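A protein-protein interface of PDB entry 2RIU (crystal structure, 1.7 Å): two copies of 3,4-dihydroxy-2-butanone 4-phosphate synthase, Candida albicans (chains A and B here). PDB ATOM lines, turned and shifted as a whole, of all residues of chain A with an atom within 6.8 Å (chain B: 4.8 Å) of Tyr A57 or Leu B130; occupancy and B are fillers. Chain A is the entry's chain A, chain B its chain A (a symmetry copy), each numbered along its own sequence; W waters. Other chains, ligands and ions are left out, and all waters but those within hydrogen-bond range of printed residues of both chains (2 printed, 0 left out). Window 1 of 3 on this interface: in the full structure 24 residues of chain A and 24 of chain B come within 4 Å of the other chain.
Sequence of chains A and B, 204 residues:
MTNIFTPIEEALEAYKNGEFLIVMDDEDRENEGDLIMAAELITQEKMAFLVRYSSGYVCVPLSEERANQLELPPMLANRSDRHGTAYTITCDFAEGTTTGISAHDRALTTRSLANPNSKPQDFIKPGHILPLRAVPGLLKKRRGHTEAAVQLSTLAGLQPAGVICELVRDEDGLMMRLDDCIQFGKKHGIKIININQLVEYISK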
ATOM      1  N   VAL A  51     -23.953  -5.607 -10.861  1.00  0.00           N
ATOM      2  CA  VAL A  51     -24.459  -4.562 -11.751  1.00  0.00           C
ATOM      3  C   VAL A  51     -25.777  -4.981 -12.410  1.00  0.00           C
ATOM      4  O   VAL A  51     -26.732  -4.205 -12.453  1.00  0.00           O
ATOM      5  CB  VAL A  51     -23.395  -4.169 -12.796  1.00  0.00           C
ATOM      6  CG1 VAL A  51     -23.982  -3.268 -13.882  1.00  0.00           C
ATOM      7  CG2 VAL A  51     -22.224  -3.491 -12.102  1.00  0.00           C
ATOM      8  N   SER A  54     -28.855  -4.659  -9.890  1.00  0.00           N
ATOM      9  CA  SER A  54     -28.844  -3.532  -8.971  1.00  0.00           C
ATOM     10  C   SER A  54     -28.956  -2.189  -9.691  1.00  0.00           C
ATOM     11  O   SER A  54     -29.054  -2.137 -10.917  1.00  0.00           O
ATOM     12  CB  SER A  54     -27.569  -3.567  -8.132  1.00  0.00           C
ATOM     13  OG  SER A  54     -26.464  -3.089  -8.884  1.00  0.00           O
ATOM     14  N   SER A  55     -28.945  -1.111  -8.913  1.00  0.00           N
ATOM     15  CA  SER A  55     -28.959   0.256  -9.435  1.00  0.00           C
ATOM     16  C   SER A  55     -27.709   0.570 -10.248  1.00  0.00           C
ATOM     17  O   SER A  55     -27.681   1.544 -11.003  1.00  0.00           O
ATOM     18  CB  SER A  55     -29.044   1.261  -8.281  1.00  0.00           C
ATOM     19  OG  SER A  55     -27.783   1.369  -7.635  1.00  0.00           O
ATOM     20  N   GLY A  56     -26.662  -0.229 -10.050  1.00  0.00           N
ATOM     21  CA  GLY A  56     -25.384  -0.014 -10.734  1.00  0.00           C
ATOM     22  C   GLY A  56     -24.523   1.087 -10.145  1.00  0.00           C
ATOM     23  O   GLY A  56     -23.395   1.298 -10.587  1.00  0.00           O
ATOM     24  N   TYR A  57     -25.045   1.788  -9.140  1.00  0.00           N
ATOM     25  CA  TYR A  57     -24.297   2.837  -8.451  1.00  0.00           C
ATOM     26  C   TYR A  57     -23.450   2.134  -7.390  1.00  0.00           C
ATOM     27  O   TYR A  57     -23.751   2.195  -6.193  1.00  0.00           O
ATOM     28  CB  TYR A  57     -25.282   3.846  -7.826  1.00  0.00           C
ATOM     29  CG  TYR A  57     -24.755   5.264  -7.640  1.00  0.00           C
ATOM     30  CD1 TYR A  57     -24.450   6.071  -8.741  1.00  0.00           C
ATOM     31  CD2 TYR A  57     -24.607   5.812  -6.367  1.00  0.00           C
ATOM     32  CE1 TYR A  57     -23.993   7.375  -8.577  1.00  0.00           C
ATOM     33  CE2 TYR A  57     -24.147   7.126  -6.191  1.00  0.00           C
ATOM     34  CZ  TYR A  57     -23.839   7.896  -7.301  1.00  0.00           C
ATOM     35  OH  TYR A  57     -23.385   9.188  -7.133  1.00  0.00           O
ATOM     36  N   VAL A  58     -22.399   1.446  -7.845  1.00  0.00           N
ATOM     37  CA  VAL A  58     -21.675   0.487  -7.005  1.00  0.00           C
ATOM     38  C   VAL A  58     -20.711   1.206  -6.080  1.00  0.00           C
ATOM     39  O   VAL A  58     -19.862   1.994  -6.532  1.00  0.00           O
ATOM     40  CB  VAL A  58     -20.932  -0.597  -7.851  1.00  0.00           C
ATOM     41  CG1 VAL A  58     -20.114  -1.516  -6.957  1.00  0.00           C
ATOM     42  CG2 VAL A  58     -21.927  -1.431  -8.656  1.00  0.00           C
ATOM     43  N   CYS A  59     -20.864   0.933  -4.784  1.00  0.00           N
ATOM     44  CA  CYS A  59     -20.110   1.602  -3.729  1.00  0.00           C
ATOM     45  C   CYS A  59     -19.189   0.649  -2.982  1.00  0.00           C
ATOM     46  O   CYS A  59     -19.483  -0.536  -2.857  1.00  0.00           O
ATOM     47  CB  CYS A  59     -21.068   2.242  -2.731  1.00  0.00           C
ATOM     48  SG  CYS A  59     -22.014   3.615  -3.405  1.00  0.00           S
ATOM     49  N   MET A  75     -16.110  13.575  -0.540  1.00  0.00           N
ATOM     50  CA  MET A  75     -16.371  14.276  -1.785  1.00  0.00           C
ATOM     51  C   MET A  75     -16.654  15.747  -1.509  1.00  0.00           C
ATOM     52  O   MET A  75     -16.213  16.622  -2.262  1.00  0.00           O
ATOM     53  CB  MET A  75     -17.537  13.634  -2.517  1.00  0.00           C
ATOM     54  CG  MET A  75     -17.667  14.077  -3.948  1.00  0.00           C
ATOM     55  SD  MET A  75     -19.160  13.372  -4.641  1.00  0.00           S
ATOM     56  CE  MET A  75     -18.640  11.683  -4.982  1.00  0.00           C
ATOM     57  N   TYR A  87     -19.741   9.615   0.896  1.00  0.00           N
ATOM     58  CA  TYR A  87     -18.992   9.426  -0.345  1.00  0.00           C
ATOM     59  C   TYR A  87     -17.632  10.108  -0.297  1.00  0.00           C
ATOM     60  O   TYR A  87     -17.515  11.241   0.183  1.00  0.00           O
ATOM     61  CB  TYR A  87     -19.773   9.995  -1.534  1.00  0.00           C
ATOM     62  CG  TYR A  87     -21.114   9.360  -1.758  1.00  0.00           C
ATOM     63  CD1 TYR A  87     -22.283   9.989  -1.325  1.00  0.00           C
ATOM     64  CD2 TYR A  87     -21.224   8.125  -2.404  1.00  0.00           C
ATOM     65  CE1 TYR A  87     -23.528   9.404  -1.529  1.00  0.00           C
ATOM     66  CE2 TYR A  87     -22.466   7.527  -2.608  1.00  0.00           C
ATOM     67  CZ  TYR A  87     -23.612   8.179  -2.170  1.00  0.00           C
ATOM     68  OH  TYR A  87     -24.838   7.595  -2.372  1.00  0.00           O
ATOM     69  N   THR A  90     -14.458   9.822  -6.179  1.00  0.00           N
ATOM     70  CA  THR A  90     -14.503   8.536  -6.886  1.00  0.00           C
ATOM     71  C   THR A  90     -13.125   8.162  -7.419  1.00  0.00           C
ATOM     72  O   THR A  90     -12.232   9.005  -7.476  1.00  0.00           O
ATOM     73  CB  THR A  90     -15.516   8.566  -8.039  1.00  0.00           C
ATOM     74  OG1 THR A  90     -15.162   9.613  -8.953  1.00  0.00           O
ATOM     75  CG2 THR A  90     -16.921   8.811  -7.503  1.00  0.00           C
ATOM     76  N   ARG A 106     -14.205  -2.282 -12.644  1.00  0.00           N
ATOM     77  CA  ARG A 106     -14.830  -2.028 -11.349  1.00  0.00           C
ATOM     78  C   ARG A 106     -14.456  -3.070 -10.302  1.00  0.00           C
ATOM     79  O   ARG A 106     -14.201  -2.724  -9.153  1.00  0.00           O
ATOM     80  CB  ARG A 106     -16.348  -1.844 -11.464  1.00  0.00           C
ATOM     81  CG  ARG A 106     -16.699  -0.485 -12.050  1.00  0.00           C
ATOM     82  CD  ARG A 106     -18.081  -0.017 -11.649  1.00  0.00           C
ATOM     83  NE  ARG A 106     -19.100  -0.458 -12.599  1.00  0.00           N
ATOM     84  CZ  ARG A 106     -20.384  -0.106 -12.523  1.00  0.00           C
ATOM     85  NH1 ARG A 106     -20.799   0.694 -11.547  1.00  0.00           N
ATOM     86  NH2 ARG A 106     -21.251  -0.539 -13.432  1.00  0.00           N
ATOM     87  N   GLY A 127     -13.063   8.693 -10.792  1.00  0.00           N
ATOM     88  CA  GLY A 127     -13.150   7.414 -11.478  1.00  0.00           C
ATOM     89  C   GLY A 127     -14.555   6.866 -11.495  1.00  0.00           C
ATOM     90  O   GLY A 127     -15.521   7.625 -11.517  1.00  0.00           O
ATOM     91  N   LEU A 130     -17.328   4.272  -6.300  1.00  0.00           N
ATOM     92  CA  LEU A 130     -17.697   5.198  -5.220  1.00  0.00           C
ATOM     93  C   LEU A 130     -17.304   4.650  -3.833  1.00  0.00           C
ATOM     94  O   LEU A 130     -18.079   3.916  -3.220  1.00  0.00           O
ATOM     95  CB  LEU A 130     -19.211   5.451  -5.255  1.00  0.00           C
ATOM     96  CG  LEU A 130     -19.793   6.153  -6.486  1.00  0.00           C
ATOM     97  CD1 LEU A 130     -21.001   5.379  -7.003  1.00  0.00           C
ATOM     98  CD2 LEU A 130     -20.152   7.604  -6.185  1.00  0.00           C
ATOM     99  N   ILE A 164     -21.072  -2.871  -2.271  1.00  0.00           N
ATOM    100  CA  ILE A 164     -22.522  -2.886  -2.078  1.00  0.00           C
ATOM    101  C   ILE A 164     -23.277  -2.245  -3.234  1.00  0.00           C
ATOM    102  O   ILE A 164     -22.752  -1.367  -3.915  1.00  0.00           O
ATOM    103  CB  ILE A 164     -22.935  -2.167  -0.759  1.00  0.00           C
ATOM    104  CG1 ILE A 164     -22.705  -0.649  -0.837  1.00  0.00           C
ATOM    105  CG2 ILE A 164     -22.203  -2.764   0.449  1.00  0.00           C
ATOM    106  CD1 ILE A 164     -23.091   0.105   0.446  1.00  0.00           C
ATOM    107  N   CYS A 165     -24.515  -2.686  -3.439  1.00  0.00           N
ATOM    108  CA  CYS A 165     -25.426  -1.997  -4.353  1.00  0.00           C
ATOM    109  C   CYS A 165     -26.852  -2.446  -4.088  1.00  0.00           C
ATOM    110  O   CYS A 165     -27.074  -3.552  -3.591  1.00  0.00           O
ATOM    111  CB  CYS A 165     -25.047  -2.242  -5.820  1.00  0.00           C
ATOM    112  SG  CYS A 165     -25.559  -0.876  -6.908  1.00  0.00           S
ATOM    113  N   GLU A 166     -27.804  -1.581  -4.429  1.00  0.00           N
ATOM    114  CA  GLU A 166     -29.227  -1.801  -4.141  1.00  0.00           C
ATOM    115  C   GLU A 166     -29.897  -2.688  -5.177  1.00  0.00           C
ATOM    116  O   GLU A 166     -29.826  -2.403  -6.372  1.00  0.00           O
ATOM    117  CB  GLU A 166     -29.973  -0.462  -4.126  1.00  0.00           C
ATOM    118  CG  GLU A 166     -29.419   0.588  -3.191  1.00  0.00           C
ATOM    119  CD  GLU A 166     -28.440   1.551  -3.855  1.00  0.00           C
ATOM    120  OE1 GLU A 166     -27.869   1.240  -4.929  1.00  0.00           O
ATOM    121  OE2 GLU A 166     -28.239   2.632  -3.274  1.00  0.00           O
ATOM    122  N   GLY B  56     -25.532   1.492 -15.038  1.00  0.00           N
ATOM    123  CA  GLY B  56     -26.209   2.149 -13.917  1.00  0.00           C
ATOM    124  C   GLY B  56     -25.482   3.354 -13.351  1.00  0.00           C
ATOM    125  O   GLY B  56     -25.998   4.031 -12.463  1.00  0.00           O
ATOM    126  N   TYR B  57     -24.286   3.632 -13.865  1.00  0.00           N
ATOM    127  CA  TYR B  57     -23.509   4.796 -13.445  1.00  0.00           C
ATOM    128  C   TYR B  57     -24.027   5.977 -14.266  1.00  0.00           C
ATOM    129  O   TYR B  57     -23.364   6.442 -15.200  1.00  0.00           O
ATOM    130  CB  TYR B  57     -22.010   4.534 -13.697  1.00  0.00           C
ATOM    131  CG  TYR B  57     -21.041   5.288 -12.793  1.00  0.00           C
ATOM    132  CD1 TYR B  57     -20.974   5.021 -11.423  1.00  0.00           C
ATOM    133  CD2 TYR B  57     -20.161   6.233 -13.319  1.00  0.00           C
ATOM    134  CE1 TYR B  57     -20.074   5.688 -10.598  1.00  0.00           C
ATOM    135  CE2 TYR B  57     -19.249   6.912 -12.496  1.00  0.00           C
ATOM    136  CZ  TYR B  57     -19.216   6.635 -11.139  1.00  0.00           C
ATOM    137  OH  TYR B  57     -18.322   7.301 -10.325  1.00  0.00           O
ATOM    138  N   VAL B  58     -25.232   6.442 -13.923  1.00  0.00           N
ATOM    139  CA  VAL B  58     -25.987   7.355 -14.786  1.00  0.00           C
ATOM    140  C   VAL B  58     -25.477   8.777 -14.639  1.00  0.00           C
ATOM    141  O   VAL B  58     -25.411   9.318 -13.521  1.00  0.00           O
ATOM    142  CB  VAL B  58     -27.525   7.285 -14.518  1.00  0.00           C
ATOM    143  CG1 VAL B  58     -28.270   8.311 -15.359  1.00  0.00           C
ATOM    144  CG2 VAL B  58     -28.065   5.890 -14.831  1.00  0.00           C
ATOM    145  N   CYS B  59     -25.108   9.364 -15.778  1.00  0.00           N
ATOM    146  CA  CYS B  59     -24.491  10.685 -15.835  1.00  0.00           C
ATOM    147  C   CYS B  59     -25.368  11.702 -16.550  1.00  0.00           C
ATOM    148  O   CYS B  59     -26.131  11.352 -17.444  1.00  0.00           O
ATOM    149  CB  CYS B  59     -23.150  10.602 -16.554  1.00  0.00           C
ATOM    150  SG  CYS B  59     -21.898   9.674 -15.657  1.00  0.00           S
ATOM    151  N   VAL B  60     -25.235  12.967 -16.160  1.00  0.00           N
ATOM    152  CA  VAL B  60     -26.036  14.045 -16.743  1.00  0.00           C
ATOM    153  C   VAL B  60     -25.136  15.163 -17.304  1.00  0.00           C
ATOM    154  O   VAL B  60     -24.763  16.081 -16.580  1.00  0.00           O
ATOM    155  CB  VAL B  60     -27.069  14.603 -15.725  1.00  0.00           C
ATOM    156  CG1 VAL B  60     -27.858  15.755 -16.314  1.00  0.00           C
ATOM    157  CG2 VAL B  60     -28.027  13.498 -15.278  1.00  0.00           C
ATOM    158  N   MET B  75     -15.458  17.636  -9.542  1.00  0.00           N
ATOM    159  CA  MET B  75     -15.279  16.816  -8.356  1.00  0.00           C
ATOM    160  C   MET B  75     -13.866  16.985  -7.811  1.00  0.00           C
ATOM    161  O   MET B  75     -13.667  17.039  -6.592  1.00  0.00           O
ATOM    162  CB  MET B  75     -15.559  15.359  -8.677  1.00  0.00           C
ATOM    163  CG  MET B  75     -15.719  14.493  -7.457  1.00  0.00           C
ATOM    164  SD  MET B  75     -15.887  12.787  -7.973  1.00  0.00           S
ATOM    165  CE  MET B  75     -17.606  12.735  -8.504  1.00  0.00           C
ATOM    166  N   TYR B  87     -16.410  14.942 -14.312  1.00  0.00           N
ATOM    167  CA  TYR B  87     -17.395  14.789 -13.243  1.00  0.00           C
ATOM    168  C   TYR B  87     -17.443  16.011 -12.337  1.00  0.00           C
ATOM    169  O   TYR B  87     -16.399  16.564 -11.972  1.00  0.00           O
ATOM    170  CB  TYR B  87     -17.065  13.565 -12.382  1.00  0.00           C
ATOM    171  CG  TYR B  87     -17.058  12.263 -13.128  1.00  0.00           C
ATOM    172  CD1 TYR B  87     -15.856  11.682 -13.537  1.00  0.00           C
ATOM    173  CD2 TYR B  87     -18.252  11.604 -13.431  1.00  0.00           C
ATOM    174  CE1 TYR B  87     -15.844  10.476 -14.230  1.00  0.00           C
ATOM    175  CE2 TYR B  87     -18.252  10.399 -14.131  1.00  0.00           C
ATOM    176  CZ  TYR B  87     -17.040   9.842 -14.521  1.00  0.00           C
ATOM    177  OH  TYR B  87     -17.035   8.653 -15.208  1.00  0.00           O
ATOM    178  N   THR B  90     -21.454  15.083  -7.063  1.00  0.00           N
ATOM    179  CA  THR B  90     -22.742  14.432  -7.327  1.00  0.00           C
ATOM    180  C   THR B  90     -23.875  15.162  -6.615  1.00  0.00           C
ATOM    181  O   THR B  90     -23.627  15.976  -5.728  1.00  0.00           O
ATOM    182  CB  THR B  90     -22.723  12.958  -6.897  1.00  0.00           C
ATOM    183  OG1 THR B  90     -22.412  12.876  -5.499  1.00  0.00           O
ATOM    184  CG2 THR B  90     -21.681  12.187  -7.697  1.00  0.00           C
ATOM    185  N   ILE B 101     -31.610   7.354  -5.119  1.00  0.00           N
ATOM    186  CA  ILE B 101     -31.165   6.336  -6.082  1.00  0.00           C
ATOM    187  C   ILE B 101     -32.291   5.716  -6.922  1.00  0.00           C
ATOM    188  O   ILE B 101     -32.037   5.148  -7.992  1.00  0.00           O
ATOM    189  CB  ILE B 101     -30.331   5.231  -5.366  1.00  0.00           C
ATOM    190  CG1 ILE B 101     -29.566   4.356  -6.375  1.00  0.00           C
ATOM    191  CG2 ILE B 101     -31.209   4.394  -4.445  1.00  0.00           C
ATOM    192  CD1 ILE B 101     -28.516   5.118  -7.171  1.00  0.00           C
ATOM    193  N   ARG B 106     -33.816   9.603  -9.409  1.00  0.00           N
ATOM    194  CA  ARG B 106     -32.814   9.897 -10.429  1.00  0.00           C
ATOM    195  C   ARG B 106     -33.395  10.638 -11.627  1.00  0.00           C
ATOM    196  O   ARG B 106     -32.775  11.564 -12.139  1.00  0.00           O
ATOM    197  CB  ARG B 106     -32.029   8.647 -10.848  1.00  0.00           C
ATOM    198  CG  ARG B 106     -31.021   8.243  -9.783  1.00  0.00           C
ATOM    199  CD  ARG B 106     -29.865   7.448 -10.349  1.00  0.00           C
ATOM    200  NE  ARG B 106     -30.139   6.012 -10.339  1.00  0.00           N
ATOM    201  CZ  ARG B 106     -29.249   5.087 -10.702  1.00  0.00           C
ATOM    202  NH1 ARG B 106     -28.033   5.450 -11.095  1.00  0.00           N
ATOM    203  NH2 ARG B 106     -29.567   3.798 -10.656  1.00  0.00           N
ATOM    204  N   GLY B 127     -24.828  13.337  -3.890  1.00  0.00           N
ATOM    205  CA  GLY B 127     -26.084  12.666  -4.181  1.00  0.00           C
ATOM    206  C   GLY B 127     -25.896  11.447  -5.049  1.00  0.00           C
ATOM    207  O   GLY B 127     -24.864  10.784  -4.980  1.00  0.00           O
ATOM    208  N   HIS B 128     -26.893  11.166  -5.882  1.00  0.00           N
ATOM    209  CA  HIS B 128     -26.923   9.909  -6.622  1.00  0.00           C
ATOM    210  C   HIS B 128     -26.927  10.071  -8.134  1.00  0.00           C
ATOM    211  O   HIS B 128     -27.000   9.074  -8.861  1.00  0.00           O
ATOM    212  CB  HIS B 128     -28.103   9.062  -6.153  1.00  0.00           C
ATOM    213  CG  HIS B 128     -28.027   8.694  -4.705  1.00  0.00           C
ATOM    214  ND1 HIS B 128     -28.425   9.548  -3.700  1.00  0.00           N
ATOM    215  CD2 HIS B 128     -27.580   7.571  -4.093  1.00  0.00           C
ATOM    216  CE1 HIS B 128     -28.231   8.965  -2.530  1.00  0.00           C
ATOM    217  NE2 HIS B 128     -27.718   7.767  -2.740  1.00  0.00           N
ATOM    218  N   ILE B 129     -26.857  11.320  -8.597  1.00  0.00           N
ATOM    219  CA  ILE B 129     -26.652  11.617 -10.015  1.00  0.00           C
ATOM    220  C   ILE B 129     -25.268  12.219 -10.234  1.00  0.00           C
ATOM    221  O   ILE B 129     -24.785  13.003  -9.404  1.00  0.00           O
ATOM    222  CB  ILE B 129     -27.766  12.561 -10.580  1.00  0.00           C
ATOM    223  CG1 ILE B 129     -29.025  11.768 -10.951  1.00  0.00           C
ATOM    224  CG2 ILE B 129     -27.284  13.366 -11.785  1.00  0.00           C
ATOM    225  CD1 ILE B 129     -28.891  10.798 -12.116  1.00  0.00           C
ATOM    226  N   LEU B 130     -24.641  11.838 -11.349  1.00  0.00           N
ATOM    227  CA  LEU B 130     -23.303  12.317 -11.724  1.00  0.00           C
ATOM    228  C   LEU B 130     -23.363  13.350 -12.869  1.00  0.00           C
ATOM    229  O   LEU B 130     -23.355  12.971 -14.040  1.00  0.00           O
ATOM    230  CB  LEU B 130     -22.433  11.129 -12.158  1.00  0.00           C
ATOM    231  CG  LEU B 130     -22.104  10.061 -11.110  1.00  0.00           C
ATOM    232  CD1 LEU B 130     -22.384   8.674 -11.677  1.00  0.00           C
ATOM    233  CD2 LEU B 130     -20.663  10.181 -10.624  1.00  0.00           C
ATOM    234  N   PRO B 131     -23.426  14.659 -12.542  1.00  0.00           N
ATOM    235  CA  PRO B 131     -23.414  15.647 -13.619  1.00  0.00           C
ATOM    236  C   PRO B 131     -22.029  15.725 -14.252  1.00  0.00           C
ATOM    237  O   PRO B 131     -21.026  15.497 -13.571  1.00  0.00           O
ATOM    238  CB  PRO B 131     -23.746  16.978 -12.901  1.00  0.00           C
ATOM    239  CG  PRO B 131     -24.254  16.578 -11.530  1.00  0.00           C
ATOM    240  CD  PRO B 131     -23.506  15.306 -11.222  1.00  0.00           C
ATOM    241  N   LEU B 132     -21.991  16.037 -15.546  1.00  0.00           N
ATOM    242  CA  LEU B 132     -20.744  16.147 -16.295  1.00  0.00           C
ATOM    243  C   LEU B 132     -20.690  17.508 -16.963  1.00  0.00           C
ATOM    244  O   LEU B 132     -21.710  18.025 -17.417  1.00  0.00           O
ATOM    245  CB  LEU B 132     -20.660  15.065 -17.370  1.00  0.00           C
ATOM    246  CG  LEU B 132     -20.876  13.612 -16.954  1.00  0.00           C
ATOM    247  CD1 LEU B 132     -20.747  12.704 -18.173  1.00  0.00           C
ATOM    248  CD2 LEU B 132     -19.887  13.216 -15.871  1.00  0.00           C
HETATM  249  O   HOH W   1     -22.136  10.233  -4.788  1.00  0.00           O
HETATM  250  O   HOH W   2     -17.112   9.827 -10.882  1.00  0.00           O
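CA of Gly B56 touches CA of Gly A56 (3.9 Å). Tyr A57 touches Thr B90. Ile B101 touches Tyr A57 (CD1 to CB, 3.5 Å). O of His B128 touches CE1 of Tyr A57, at 3.5 Å. Tyr A57 touches Leu B130. CE of Met B75 touches CE of Met A75, 3.8 Å away. Thr A90 touches Tyr B57 (CG2 to OH, 3.5 Å). Gly A127 touches Tyr B87. Leu A130 touches Tyr B57 (CD1 to CE1, 3.7 Å). Ile B101 touches Glu A166.
Tyr A57 touches Thr B90, and with the chains exchanged Thr A90 touches Tyr B57. Tyr A57 touches Gly B127, and with the chains exchanged Gly A127 touches Tyr B57. Tyr A57 touches Leu B130, and with the chains exchanged Leu A130 touches Tyr B57. Tyr A87 touches Gly B127, and with the chains exchanged Gly A127 touches Tyr B87. 10 positions are printed for both chains. Of the 19 pairs that touch across the chains among the printed residues, 12 have their exchanged pair printed and touching as well.
The guanidinium group of Arg B106 sits at hydrogen-bond distance from the backbone carbonyl oxygen of Ser A55. The side-chain hydroxyl of Tyr A57 sits at hydrogen-bond distance from the backbone carbonyl oxygen of Gly B127. OG1 of Thr B90 lies within hydrogen-bond range of SD of Met A75 (3.4 Å). The side-chain hydroxyl (OH) of Tyr A87 lies within hydrogen-bond range of a ring nitrogen (NE2) of His B128 (2.9 Å). The side-chain sulfur (SD) of Met B75 sits at hydrogen-bond distance from the side-chain hydroxyl (OG1) of Thr A90 (3.4 Å). O of Gly A127 sits at hydrogen-bond distance from OH of Tyr B57 (3.1 Å). The backbone carbonyl oxygen (O) of Ser A55 lies close to the backbone carbonyl oxygen (O) of Gly B56.
Of chain B, only Thr B90 (3.5 Å), Ile B101 (3.5 Å), Gly B127 (3.1 Å), His B128 (3.5 Å) and Leu B130 (3.7 Å) come within 4 Å of Tyr A57. Of chain A, only Tyr A57 (3.7 Å) comes within 4 Å of Leu B130. Printed residues of chain B within 4 Å of Gly A127: Tyr B57 (3.1 Å) and Tyr B87 (3.9 Å). Of the printed residues of chain B, Met A75 touches Met B75 and Thr B90. Of the printed residues of chain B, Thr A90 touches Tyr B57 and Met B75. Of the printed residues of chain A, Tyr B87 touches Gly A127. Val A51 touches none of the printed residues of chain B. The nearest residue of chain A that does not touch Leu B130 is Thr A90 (5.1 Å).
Hydrophobic or aromatic side chains of chain A within 4 Å of the printed part of chain B: Tyr A57, Met A75, Tyr A87 and Leu A130. Of the 16 printed residues of chain B, 10 touch a printed residue of chain A. Hydrophobic or aromatic side chains of chain B within 4 Å of the printed part of chain A: Tyr B57, Met B75, Tyr B87, Ile B101, His B128 and Leu B130. Among the printed residues, 19 pairs touch across the chains.
The side-chain carboxylate (OE1) of Glu A166 lies within hydrogen-bond range of the side-chain hydroxyl (OG) of Ser A55. The backbone carbonyl oxygen (O) of Gly A56 sits at hydrogen-bond distance from the guanidinium group (NH1) of Arg A106 (2.8 Å). The backbone carbonyl oxygen of Tyr A57 lies within hydrogen-bond range of the side-chain sulfur of Cys A59, 3.6 Å away. O of Tyr A87 lies within hydrogen-bond range of N of Met A75 (2.8 Å). SG of Cys A165 sits at hydrogen-bond distance from OE1 of Glu A166 (3.7 Å). O of Val B58 is in hydrogen-bond range of N of Leu B130, at 3.4 Å.
Water W1 lies within hydrogen-bond range of OG1 of Thr B90, O of Gly B127 and OH of Tyr A57. Water W2 lies within hydrogen-bond range of OG1 of Thr A90 (2.8 Å), O of Gly A127 (2.8 Å) and OH of Tyr B57 (2.9 Å).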
